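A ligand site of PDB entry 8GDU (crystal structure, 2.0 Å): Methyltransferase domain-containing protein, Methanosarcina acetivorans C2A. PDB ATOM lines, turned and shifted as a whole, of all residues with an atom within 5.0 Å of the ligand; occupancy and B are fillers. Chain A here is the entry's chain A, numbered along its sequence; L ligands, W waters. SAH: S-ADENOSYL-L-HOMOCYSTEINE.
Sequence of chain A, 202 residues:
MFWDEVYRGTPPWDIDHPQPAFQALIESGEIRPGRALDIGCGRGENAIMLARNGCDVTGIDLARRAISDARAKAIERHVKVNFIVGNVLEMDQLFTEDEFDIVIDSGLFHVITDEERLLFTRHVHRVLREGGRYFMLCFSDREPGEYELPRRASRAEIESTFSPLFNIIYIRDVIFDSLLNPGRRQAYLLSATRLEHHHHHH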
ATOM      1  N   TRP A   3      25.511  10.179  -1.071  1.00  0.00           N
ATOM      2  CA  TRP A   3      24.688   9.078  -0.572  1.00  0.00           C
ATOM      3  C   TRP A   3      25.344   8.364   0.615  1.00  0.00           C
ATOM      4  O   TRP A   3      24.629   7.815   1.459  1.00  0.00           O
ATOM      5  CB  TRP A   3      24.354   8.119  -1.717  1.00  0.00           C
ATOM      6  CG  TRP A   3      23.473   8.821  -2.721  1.00  0.00           C
ATOM      7  CD1 TRP A   3      23.869   9.337  -3.934  1.00  0.00           C
ATOM      8  CD2 TRP A   3      22.100   9.181  -2.553  1.00  0.00           C
ATOM      9  NE1 TRP A   3      22.803   9.957  -4.547  1.00  0.00           N
ATOM     10  CE2 TRP A   3      21.707   9.879  -3.716  1.00  0.00           C
ATOM     11  CE3 TRP A   3      21.155   8.969  -1.535  1.00  0.00           C
ATOM     12  CZ2 TRP A   3      20.402  10.356  -3.909  1.00  0.00           C
ATOM     13  CZ3 TRP A   3      19.853   9.460  -1.721  1.00  0.00           C
ATOM     14  CH2 TRP A   3      19.497  10.147  -2.898  1.00  0.00           C
ATOM     15  N   TYR A   7      23.240   8.030   4.523  1.00  0.00           N
ATOM     16  CA  TYR A   7      23.092   6.822   5.330  1.00  0.00           C
ATOM     17  C   TYR A   7      23.943   6.832   6.592  1.00  0.00           C
ATOM     18  O   TYR A   7      23.973   5.819   7.307  1.00  0.00           O
ATOM     19  CB  TYR A   7      23.383   5.590   4.474  1.00  0.00           C
ATOM     20  CG  TYR A   7      22.213   5.346   3.549  1.00  0.00           C
ATOM     21  CD1 TYR A   7      20.994   4.906   4.053  1.00  0.00           C
ATOM     22  CD2 TYR A   7      22.311   5.605   2.182  1.00  0.00           C
ATOM     23  CE1 TYR A   7      19.912   4.695   3.226  1.00  0.00           C
ATOM     24  CE2 TYR A   7      21.217   5.386   1.328  1.00  0.00           C
ATOM     25  CZ  TYR A   7      20.026   4.937   1.868  1.00  0.00           C
ATOM     26  OH  TYR A   7      18.940   4.724   1.033  1.00  0.00           O
ATOM     27  N   TRP A  13      12.784   8.178   3.937  1.00  0.00           N
ATOM     28  CA  TRP A  13      12.239   6.987   3.295  1.00  0.00           C
ATOM     29  C   TRP A  13      12.667   5.704   3.991  1.00  0.00           C
ATOM     30  O   TRP A  13      12.236   4.623   3.582  1.00  0.00           O
ATOM     31  CB  TRP A  13      12.678   6.908   1.829  1.00  0.00           C
ATOM     32  CG  TRP A  13      14.174   6.878   1.645  1.00  0.00           C
ATOM     33  CD1 TRP A  13      14.994   5.789   1.678  1.00  0.00           C
ATOM     34  CD2 TRP A  13      15.018   8.009   1.389  1.00  0.00           C
ATOM     35  NE1 TRP A  13      16.296   6.174   1.459  1.00  0.00           N
ATOM     36  CE2 TRP A  13      16.336   7.525   1.293  1.00  0.00           C
ATOM     37  CE3 TRP A  13      14.779   9.380   1.262  1.00  0.00           C
ATOM     38  CZ2 TRP A  13      17.427   8.366   1.046  1.00  0.00           C
ATOM     39  CZ3 TRP A  13      15.861  10.221   1.019  1.00  0.00           C
ATOM     40  CH2 TRP A  13      17.161   9.710   0.906  1.00  0.00           C
ATOM     41  N   ASP A  14      13.501   5.790   5.022  1.00  0.00           N
ATOM     42  CA  ASP A  14      14.159   4.607   5.597  1.00  0.00           C
ATOM     43  C   ASP A  14      13.276   3.972   6.677  1.00  0.00           C
ATOM     44  O   ASP A  14      13.648   3.864   7.847  1.00  0.00           O
ATOM     45  CB  ASP A  14      15.529   4.999   6.140  1.00  0.00           C
ATOM     46  CG  ASP A  14      16.371   3.793   6.538  1.00  0.00           C
ATOM     47  OD1 ASP A  14      16.294   2.762   5.866  1.00  0.00           O
ATOM     48  OD2 ASP A  14      17.113   3.903   7.535  1.00  0.00           O
ATOM     49  N   GLN A  19       7.760  -1.007   1.387  1.00  0.00           N
ATOM     50  CA  GLN A  19       6.731  -0.091   0.909  1.00  0.00           C
ATOM     51  C   GLN A  19       5.437  -0.844   0.631  1.00  0.00           C
ATOM     52  O   GLN A  19       5.475  -1.906  -0.004  1.00  0.00           O
ATOM     53  CB  GLN A  19       7.209   0.617  -0.364  1.00  0.00           C
ATOM     54  CG  GLN A  19       8.162   1.802  -0.107  1.00  0.00           C
ATOM     55  CD  GLN A  19       7.536   2.909   0.732  1.00  0.00           C
ATOM     56  OE1 GLN A  19       6.324   3.145   0.695  1.00  0.00           O
ATOM     57  NE2 GLN A  19       8.381   3.606   1.499  1.00  0.00           N
ATOM     58  N   ASP A  38      16.555  -5.064  -7.271  1.00  0.00           N
ATOM     59  CA  ASP A  38      16.106  -3.854  -6.599  1.00  0.00           C
ATOM     60  C   ASP A  38      17.199  -2.819  -6.813  1.00  0.00           C
ATOM     61  O   ASP A  38      18.287  -2.934  -6.222  1.00  0.00           O
ATOM     62  CB  ASP A  38      15.840  -4.134  -5.116  1.00  0.00           C
ATOM     63  CG  ASP A  38      15.329  -2.911  -4.362  1.00  0.00           C
ATOM     64  OD1 ASP A  38      15.348  -1.781  -4.919  1.00  0.00           O
ATOM     65  OD2 ASP A  38      14.909  -3.069  -3.198  1.00  0.00           O
ATOM     66  N   ILE A  39      16.927  -1.822  -7.654  1.00  0.00           N
ATOM     67  CA  ILE A  39      17.927  -0.804  -7.981  1.00  0.00           C
ATOM     68  C   ILE A  39      17.822   0.354  -7.004  1.00  0.00           C
ATOM     69  O   ILE A  39      16.747   0.922  -6.804  1.00  0.00           O
ATOM     70  CB  ILE A  39      17.785  -0.326  -9.441  1.00  0.00           C
ATOM     71  CG1 ILE A  39      16.353   0.119  -9.794  1.00  0.00           C
ATOM     72  CG2 ILE A  39      18.204  -1.444 -10.400  1.00  0.00           C
ATOM     73  CD1 ILE A  39      16.280   0.726 -11.222  1.00  0.00           C
ATOM     74  N   GLY A  40      18.971   0.741  -6.418  1.00  0.00           N
ATOM     75  CA  GLY A  40      18.944   1.764  -5.391  1.00  0.00           C
ATOM     76  C   GLY A  40      18.222   1.223  -4.172  1.00  0.00           C
ATOM     77  O   GLY A  40      17.323   1.863  -3.630  1.00  0.00           O
ATOM     78  N   CYS A  41      18.604   0.013  -3.749  1.00  0.00           N
ATOM     79  CA  CYS A  41      17.833  -0.736  -2.764  1.00  0.00           C
ATOM     80  C   CYS A  41      17.922  -0.167  -1.361  1.00  0.00           C
ATOM     81  O   CYS A  41      17.162  -0.612  -0.493  1.00  0.00           O
ATOM     82  CB  CYS A  41      18.296  -2.191  -2.747  1.00  0.00           C
ATOM     83  SG  CYS A  41      20.041  -2.395  -2.231  1.00  0.00           S
ATOM     84  N   GLY A  42      18.812   0.794  -1.100  1.00  0.00           N
ATOM     85  CA  GLY A  42      18.903   1.331   0.255  1.00  0.00           C
ATOM     86  C   GLY A  42      19.180   0.245   1.279  1.00  0.00           C
ATOM     87  O   GLY A  42      19.954  -0.698   1.040  1.00  0.00           O
ATOM     88  N   ASN A  46      12.576  -3.664   0.855  1.00  0.00           N
ATOM     89  CA  ASN A  46      11.782  -4.181  -0.260  1.00  0.00           C
ATOM     90  C   ASN A  46      12.415  -5.441  -0.841  1.00  0.00           C
ATOM     91  O   ASN A  46      11.692  -6.385  -1.193  1.00  0.00           O
ATOM     92  CB  ASN A  46      11.625  -3.109  -1.356  1.00  0.00           C
ATOM     93  CG  ASN A  46      10.710  -1.973  -0.941  1.00  0.00           C
ATOM     94  OD1 ASN A  46       9.659  -2.186  -0.306  1.00  0.00           O
ATOM     95  ND2 ASN A  46      11.096  -0.751  -1.291  1.00  0.00           N
ATOM     96  N   ILE A  60      21.118  -3.513  -5.412  1.00  0.00           N
ATOM     97  CA  ILE A  60      22.285  -2.687  -5.712  1.00  0.00           C
ATOM     98  C   ILE A  60      22.068  -1.272  -5.203  1.00  0.00           C
ATOM     99  O   ILE A  60      20.970  -0.702  -5.322  1.00  0.00           O
ATOM    100  CB  ILE A  60      22.590  -2.690  -7.231  1.00  0.00           C
ATOM    101  CG1 ILE A  60      23.870  -1.911  -7.521  1.00  0.00           C
ATOM    102  CG2 ILE A  60      21.437  -2.096  -8.036  1.00  0.00           C
ATOM    103  CD1 ILE A  60      24.101  -1.719  -9.008  1.00  0.00           C
ATOM    104  N   ASP A  61      23.131  -0.692  -4.635  1.00  0.00           N
ATOM    105  CA  ASP A  61      23.092   0.665  -4.144  1.00  0.00           C
ATOM    106  C   ASP A  61      24.499   1.226  -4.155  1.00  0.00           C
ATOM    107  O   ASP A  61      25.479   0.490  -3.980  1.00  0.00           O
ATOM    108  CB  ASP A  61      22.510   0.715  -2.730  1.00  0.00           C
ATOM    109  CG  ASP A  61      21.960   2.080  -2.353  1.00  0.00           C
ATOM    110  OD1 ASP A  61      22.757   2.984  -2.033  1.00  0.00           O
ATOM    111  OD2 ASP A  61      20.724   2.250  -2.394  1.00  0.00           O
ATOM    112  N   LEU A  62      24.589   2.544  -4.356  1.00  0.00           N
ATOM    113  CA  LEU A  62      25.880   3.230  -4.352  1.00  0.00           C
ATOM    114  C   LEU A  62      26.506   3.279  -2.956  1.00  0.00           C
ATOM    115  O   LEU A  62      27.734   3.381  -2.855  1.00  0.00           O
ATOM    116  CB  LEU A  62      25.729   4.677  -4.846  1.00  0.00           C
ATOM    117  CG  LEU A  62      25.745   5.113  -6.297  1.00  0.00           C
ATOM    118  CD1 LEU A  62      25.632   6.663  -6.385  1.00  0.00           C
ATOM    119  CD2 LEU A  62      27.003   4.605  -7.016  1.00  0.00           C
ATOM    120  N   ALA A  63      25.701   3.270  -1.891  1.00  0.00           N
ATOM    121  CA  ALA A  63      26.203   3.540  -0.550  1.00  0.00           C
ATOM    122  C   ALA A  63      26.577   2.247   0.173  1.00  0.00           C
ATOM    123  O   ALA A  63      25.704   1.421   0.466  1.00  0.00           O
ATOM    124  CB  ALA A  63      25.153   4.318   0.246  1.00  0.00           C
ATOM    125  N   GLY A  86      27.162  -0.819  -5.935  1.00  0.00           N
ATOM    126  CA  GLY A  86      27.359  -0.582  -7.351  1.00  0.00           C
ATOM    127  C   GLY A  86      26.505   0.566  -7.851  1.00  0.00           C
ATOM    128  O   GLY A  86      25.610   1.058  -7.154  1.00  0.00           O
ATOM    129  N   ASN A  87      26.790   0.959  -9.093  1.00  0.00           N
ATOM    130  CA  ASN A  87      26.161   2.105  -9.750  1.00  0.00           C
ATOM    131  C   ASN A  87      25.224   1.577 -10.843  1.00  0.00           C
ATOM    132  O   ASN A  87      25.664   0.877 -11.752  1.00  0.00           O
ATOM    133  CB  ASN A  87      27.246   3.003 -10.352  1.00  0.00           C
ATOM    134  CG  ASN A  87      26.719   4.344 -10.805  1.00  0.00           C
ATOM    135  OD1 ASN A  87      25.548   4.492 -11.142  1.00  0.00           O
ATOM    136  ND2 ASN A  87      27.604   5.341 -10.825  1.00  0.00           N
ATOM    137  N   VAL A  88      23.946   1.959 -10.758  1.00  0.00           N
ATOM    138  CA  VAL A  88      22.941   1.561 -11.757  1.00  0.00           C
ATOM    139  C   VAL A  88      23.353   2.023 -13.155  1.00  0.00           C
ATOM    140  O   VAL A  88      22.984   1.396 -14.155  1.00  0.00           O
ATOM    141  CB  VAL A  88      21.550   2.089 -11.358  1.00  0.00           C
ATOM    142  CG1 VAL A  88      21.458   3.625 -11.474  1.00  0.00           C
ATOM    143  CG2 VAL A  88      20.450   1.469 -12.204  1.00  0.00           C
ATOM    144  N   LEU A  89      24.112   3.110 -13.258  1.00  0.00           N
ATOM    145  CA  LEU A  89      24.583   3.584 -14.549  1.00  0.00           C
ATOM    146  C   LEU A  89      25.814   2.839 -15.039  1.00  0.00           C
ATOM    147  O   LEU A  89      26.367   3.209 -16.075  1.00  0.00           O
ATOM    148  CB  LEU A  89      24.877   5.092 -14.489  1.00  0.00           C
ATOM    149  CG  LEU A  89      23.696   5.950 -13.986  1.00  0.00           C
ATOM    150  CD1 LEU A  89      24.048   7.434 -13.968  1.00  0.00           C
ATOM    151  CD2 LEU A  89      22.441   5.716 -14.831  1.00  0.00           C
ATOM    152  N   SER A 106      12.384   1.787  -6.016  1.00  0.00           N
ATOM    153  CA  SER A 106      11.666   2.483  -4.947  1.00  0.00           C
ATOM    154  C   SER A 106      12.406   3.789  -4.652  1.00  0.00           C
ATOM    155  O   SER A 106      13.246   3.854  -3.754  1.00  0.00           O
ATOM    156  CB  SER A 106      11.566   1.598  -3.689  1.00  0.00           C
ATOM    157  OG  SER A 106      10.834   2.269  -2.674  1.00  0.00           O
ATOM    158  N   GLY A 107      12.090   4.830  -5.418  1.00  0.00           N
ATOM    159  CA  GLY A 107      12.684   6.125  -5.180  1.00  0.00           C
ATOM    160  C   GLY A 107      14.038   6.371  -5.824  1.00  0.00           C
ATOM    161  O   GLY A 107      14.639   7.422  -5.573  1.00  0.00           O
ATOM    162  N   LEU A 108      14.542   5.458  -6.665  1.00  0.00           N
ATOM    163  CA  LEU A 108      15.791   5.728  -7.371  1.00  0.00           C
ATOM    164  C   LEU A 108      15.572   6.640  -8.584  1.00  0.00           C
ATOM    165  O   LEU A 108      16.284   7.645  -8.745  1.00  0.00           O
ATOM    166  CB  LEU A 108      16.470   4.431  -7.826  1.00  0.00           C
ATOM    167  CG  LEU A 108      17.715   4.636  -8.715  1.00  0.00           C
ATOM    168  CD1 LEU A 108      18.723   5.567  -8.044  1.00  0.00           C
ATOM    169  CD2 LEU A 108      18.374   3.285  -9.043  1.00  0.00           C
ATOM    170  N   VAL A 111      15.686  10.405  -8.144  1.00  0.00           N
ATOM    171  CA  VAL A 111      16.904  11.146  -7.840  1.00  0.00           C
ATOM    172  C   VAL A 111      17.927  11.073  -8.956  1.00  0.00           C
ATOM    173  O   VAL A 111      19.012  11.652  -8.829  1.00  0.00           O
ATOM    174  CB  VAL A 111      17.525  10.691  -6.509  1.00  0.00           C
ATOM    175  CG1 VAL A 111      16.515  10.834  -5.363  1.00  0.00           C
ATOM    176  CG2 VAL A 111      18.029   9.257  -6.596  1.00  0.00           C
ATOM    177  N   ILE A 112      17.634  10.368 -10.058  1.00  0.00           N
ATOM    178  CA  ILE A 112      18.544  10.379 -11.205  1.00  0.00           C
ATOM    179  C   ILE A 112      18.565  11.772 -11.829  1.00  0.00           C
ATOM    180  O   ILE A 112      17.513  12.361 -12.065  1.00  0.00           O
ATOM    181  CB  ILE A 112      18.111   9.314 -12.230  1.00  0.00           C
ATOM    182  CG1 ILE A 112      18.159   7.914 -11.624  1.00  0.00           C
ATOM    183  CG2 ILE A 112      18.994   9.384 -13.462  1.00  0.00           C
ATOM    184  CD1 ILE A 112      19.591   7.432 -11.295  1.00  0.00           C
HETATM  185  N   SAH L   1      14.897   1.933  -2.293  1.00  0.00           N
HETATM  186  CA  SAH L   1      15.284   2.405  -0.961  1.00  0.00           C
HETATM  187  CB  SAH L   1      16.089   3.701  -1.033  1.00  0.00           C
HETATM  188  CG  SAH L   1      15.557   4.781  -1.963  1.00  0.00           C
HETATM  189  SD  SAH L   1      16.493   6.331  -1.817  1.00  0.00           S
HETATM  190  C   SAH L   1      14.048   2.619  -0.097  1.00  0.00           C
HETATM  191  O   SAH L   1      12.939   2.563  -0.617  1.00  0.00           O
HETATM  192  OXT SAH L   1      14.175   2.846   1.118  1.00  0.00           O
HETATM  193  C5' SAH L   1      17.371   6.148  -3.403  1.00  0.00           C
HETATM  194  C4' SAH L   1      18.603   5.256  -3.306  1.00  0.00           C
HETATM  195  O4' SAH L   1      19.303   5.193  -4.530  1.00  0.00           O
HETATM  196  C3' SAH L   1      19.613   5.670  -2.246  1.00  0.00           C
HETATM  197  O3' SAH L   1      19.737   4.556  -1.395  1.00  0.00           O
HETATM  198  C2' SAH L   1      20.896   5.911  -3.049  1.00  0.00           C
HETATM  199  O2' SAH L   1      22.094   5.540  -2.409  1.00  0.00           O
HETATM  200  C1' SAH L   1      20.692   5.052  -4.270  1.00  0.00           C
HETATM  201  N9  SAH L   1      21.358   5.530  -5.468  1.00  0.00           N
HETATM  202  C8  SAH L   1      21.422   6.824  -5.923  1.00  0.00           C
HETATM  203  N7  SAH L   1      22.077   6.830  -7.102  1.00  0.00           N
HETATM  204  C5  SAH L   1      22.438   5.553  -7.410  1.00  0.00           C
HETATM  205  C6  SAH L   1      23.122   4.997  -8.482  1.00  0.00           C
HETATM  206  N6  SAH L   1      23.592   5.741  -9.478  1.00  0.00           N
HETATM  207  N1  SAH L   1      23.300   3.643  -8.515  1.00  0.00           N
HETATM  208  C2  SAH L   1      22.845   2.837  -7.485  1.00  0.00           C
HETATM  209  N3  SAH L   1      22.155   3.410  -6.426  1.00  0.00           N
HETATM  210  C4  SAH L   1      21.958   4.733  -6.387  1.00  0.00           C
HETATM  211  O   HOH W   1      14.632   0.701  -5.022  1.00  0.00           O
HETATM  212  O   HOH W   2      16.409   2.435   2.894  1.00  0.00           O
HETATM  213  O   HOH W   3      23.627   8.735  -9.784  1.00  0.00           O
HETATM  214  O   HOH W   4      13.860  -0.688  -2.239  1.00  0.00           O
HETATM  215  O   HOH W   5      11.232   2.840   1.618  1.00  0.00           O
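An oxygen (O3') of the ligand sits at hydrogen-bond distance from the side-chain hydroxyl (OH) of Tyr 7 (2.6 Å). An oxygen (O2') of the ligand is in hydrogen-bond range of the side-chain carboxylate (OD1) of Asp 61 (2.7 Å). The backbone carbonyl oxygen of Gly 40 sits at hydrogen-bond distance from a nitrogen (N) of the ligand, 2.8 Å away. The side-chain amide oxygen (OD1) of Asn 87 sits at hydrogen-bond distance from a nitrogen (N6) of the ligand (2.9 Å). A nitrogen (N1) of the ligand is in hydrogen-bond range of the backbone NH (N) of Val 88 (2.9 Å). N of the ligand lies within hydrogen-bond range of O of Ser 106 (2.9 Å). The side-chain hydroxyl (OG) of Ser 106 lies within hydrogen-bond range of an oxygen (O) of the ligand, at 3.0 Å. The indole nitrogen (NE1) of Trp 13 lies close to a sulfur (SD) of the ligand (3.3 Å). The backbone NH (N) of Leu 62 lies within hydrogen-bond range of a nitrogen (N3) of the ligand, 3.3 Å away.
The side-chain hydroxyl (OH) of Tyr 7 lies within hydrogen-bond range of the indole nitrogen (NE1) of Trp 13 (3.0 Å). N of Gly 86 sits at hydrogen-bond distance from O of Asp 61, 2.9 Å away. OD2 of Asp 61 sits at hydrogen-bond distance from N of Cys 41 (3.4 Å). N of Gly 42 lies within hydrogen-bond range of OD2 of Asp 61 (2.7 Å). The backbone NH of Ala 63 sits at hydrogen-bond distance from the side-chain carboxylate of Asp 61, at 3.0 Å. The backbone NH of Leu 89 sits at hydrogen-bond distance from the side-chain amide oxygen of Asn 87 (2.9 Å). ND2 of Asn 46 lies within hydrogen-bond range of OG of Ser 106 (3.3 Å). The backbone NH (N) of Cys 41 lies within hydrogen-bond range of the backbone carbonyl oxygen (O) of Ile 60 (2.9 Å).
Merely in contact with the ligand: Gly 86 (3.3 Å), Trp 3 (3.4 Å), Leu 108 (3.6 Å), Cys 41 (3.6 Å), Gly 107 (3.7 Å), Gly 42 (3.7 Å) and Asn 46 (3.9 Å). Of the 24 residues printed, 15 come within 4 Å of the ligand.
Water W4 lies within hydrogen-bond range of the side-chain carboxylate (OD2) of Asp 38 (2.8 Å), a nitrogen (N) of the ligand (2.8 Å) and the side-chain amide nitrogen (ND2) of Asn 46 (2.9 Å). Water W5 lies within hydrogen-bond range of an oxygen (O) of the ligand, the backbone carbonyl oxygen (O) of Trp 13 and the side-chain amide nitrogen (NE2) of Gln 19. Water W2 bridges an oxygen (OXT) of the ligand and the side-chain carboxylate of Asp 14.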
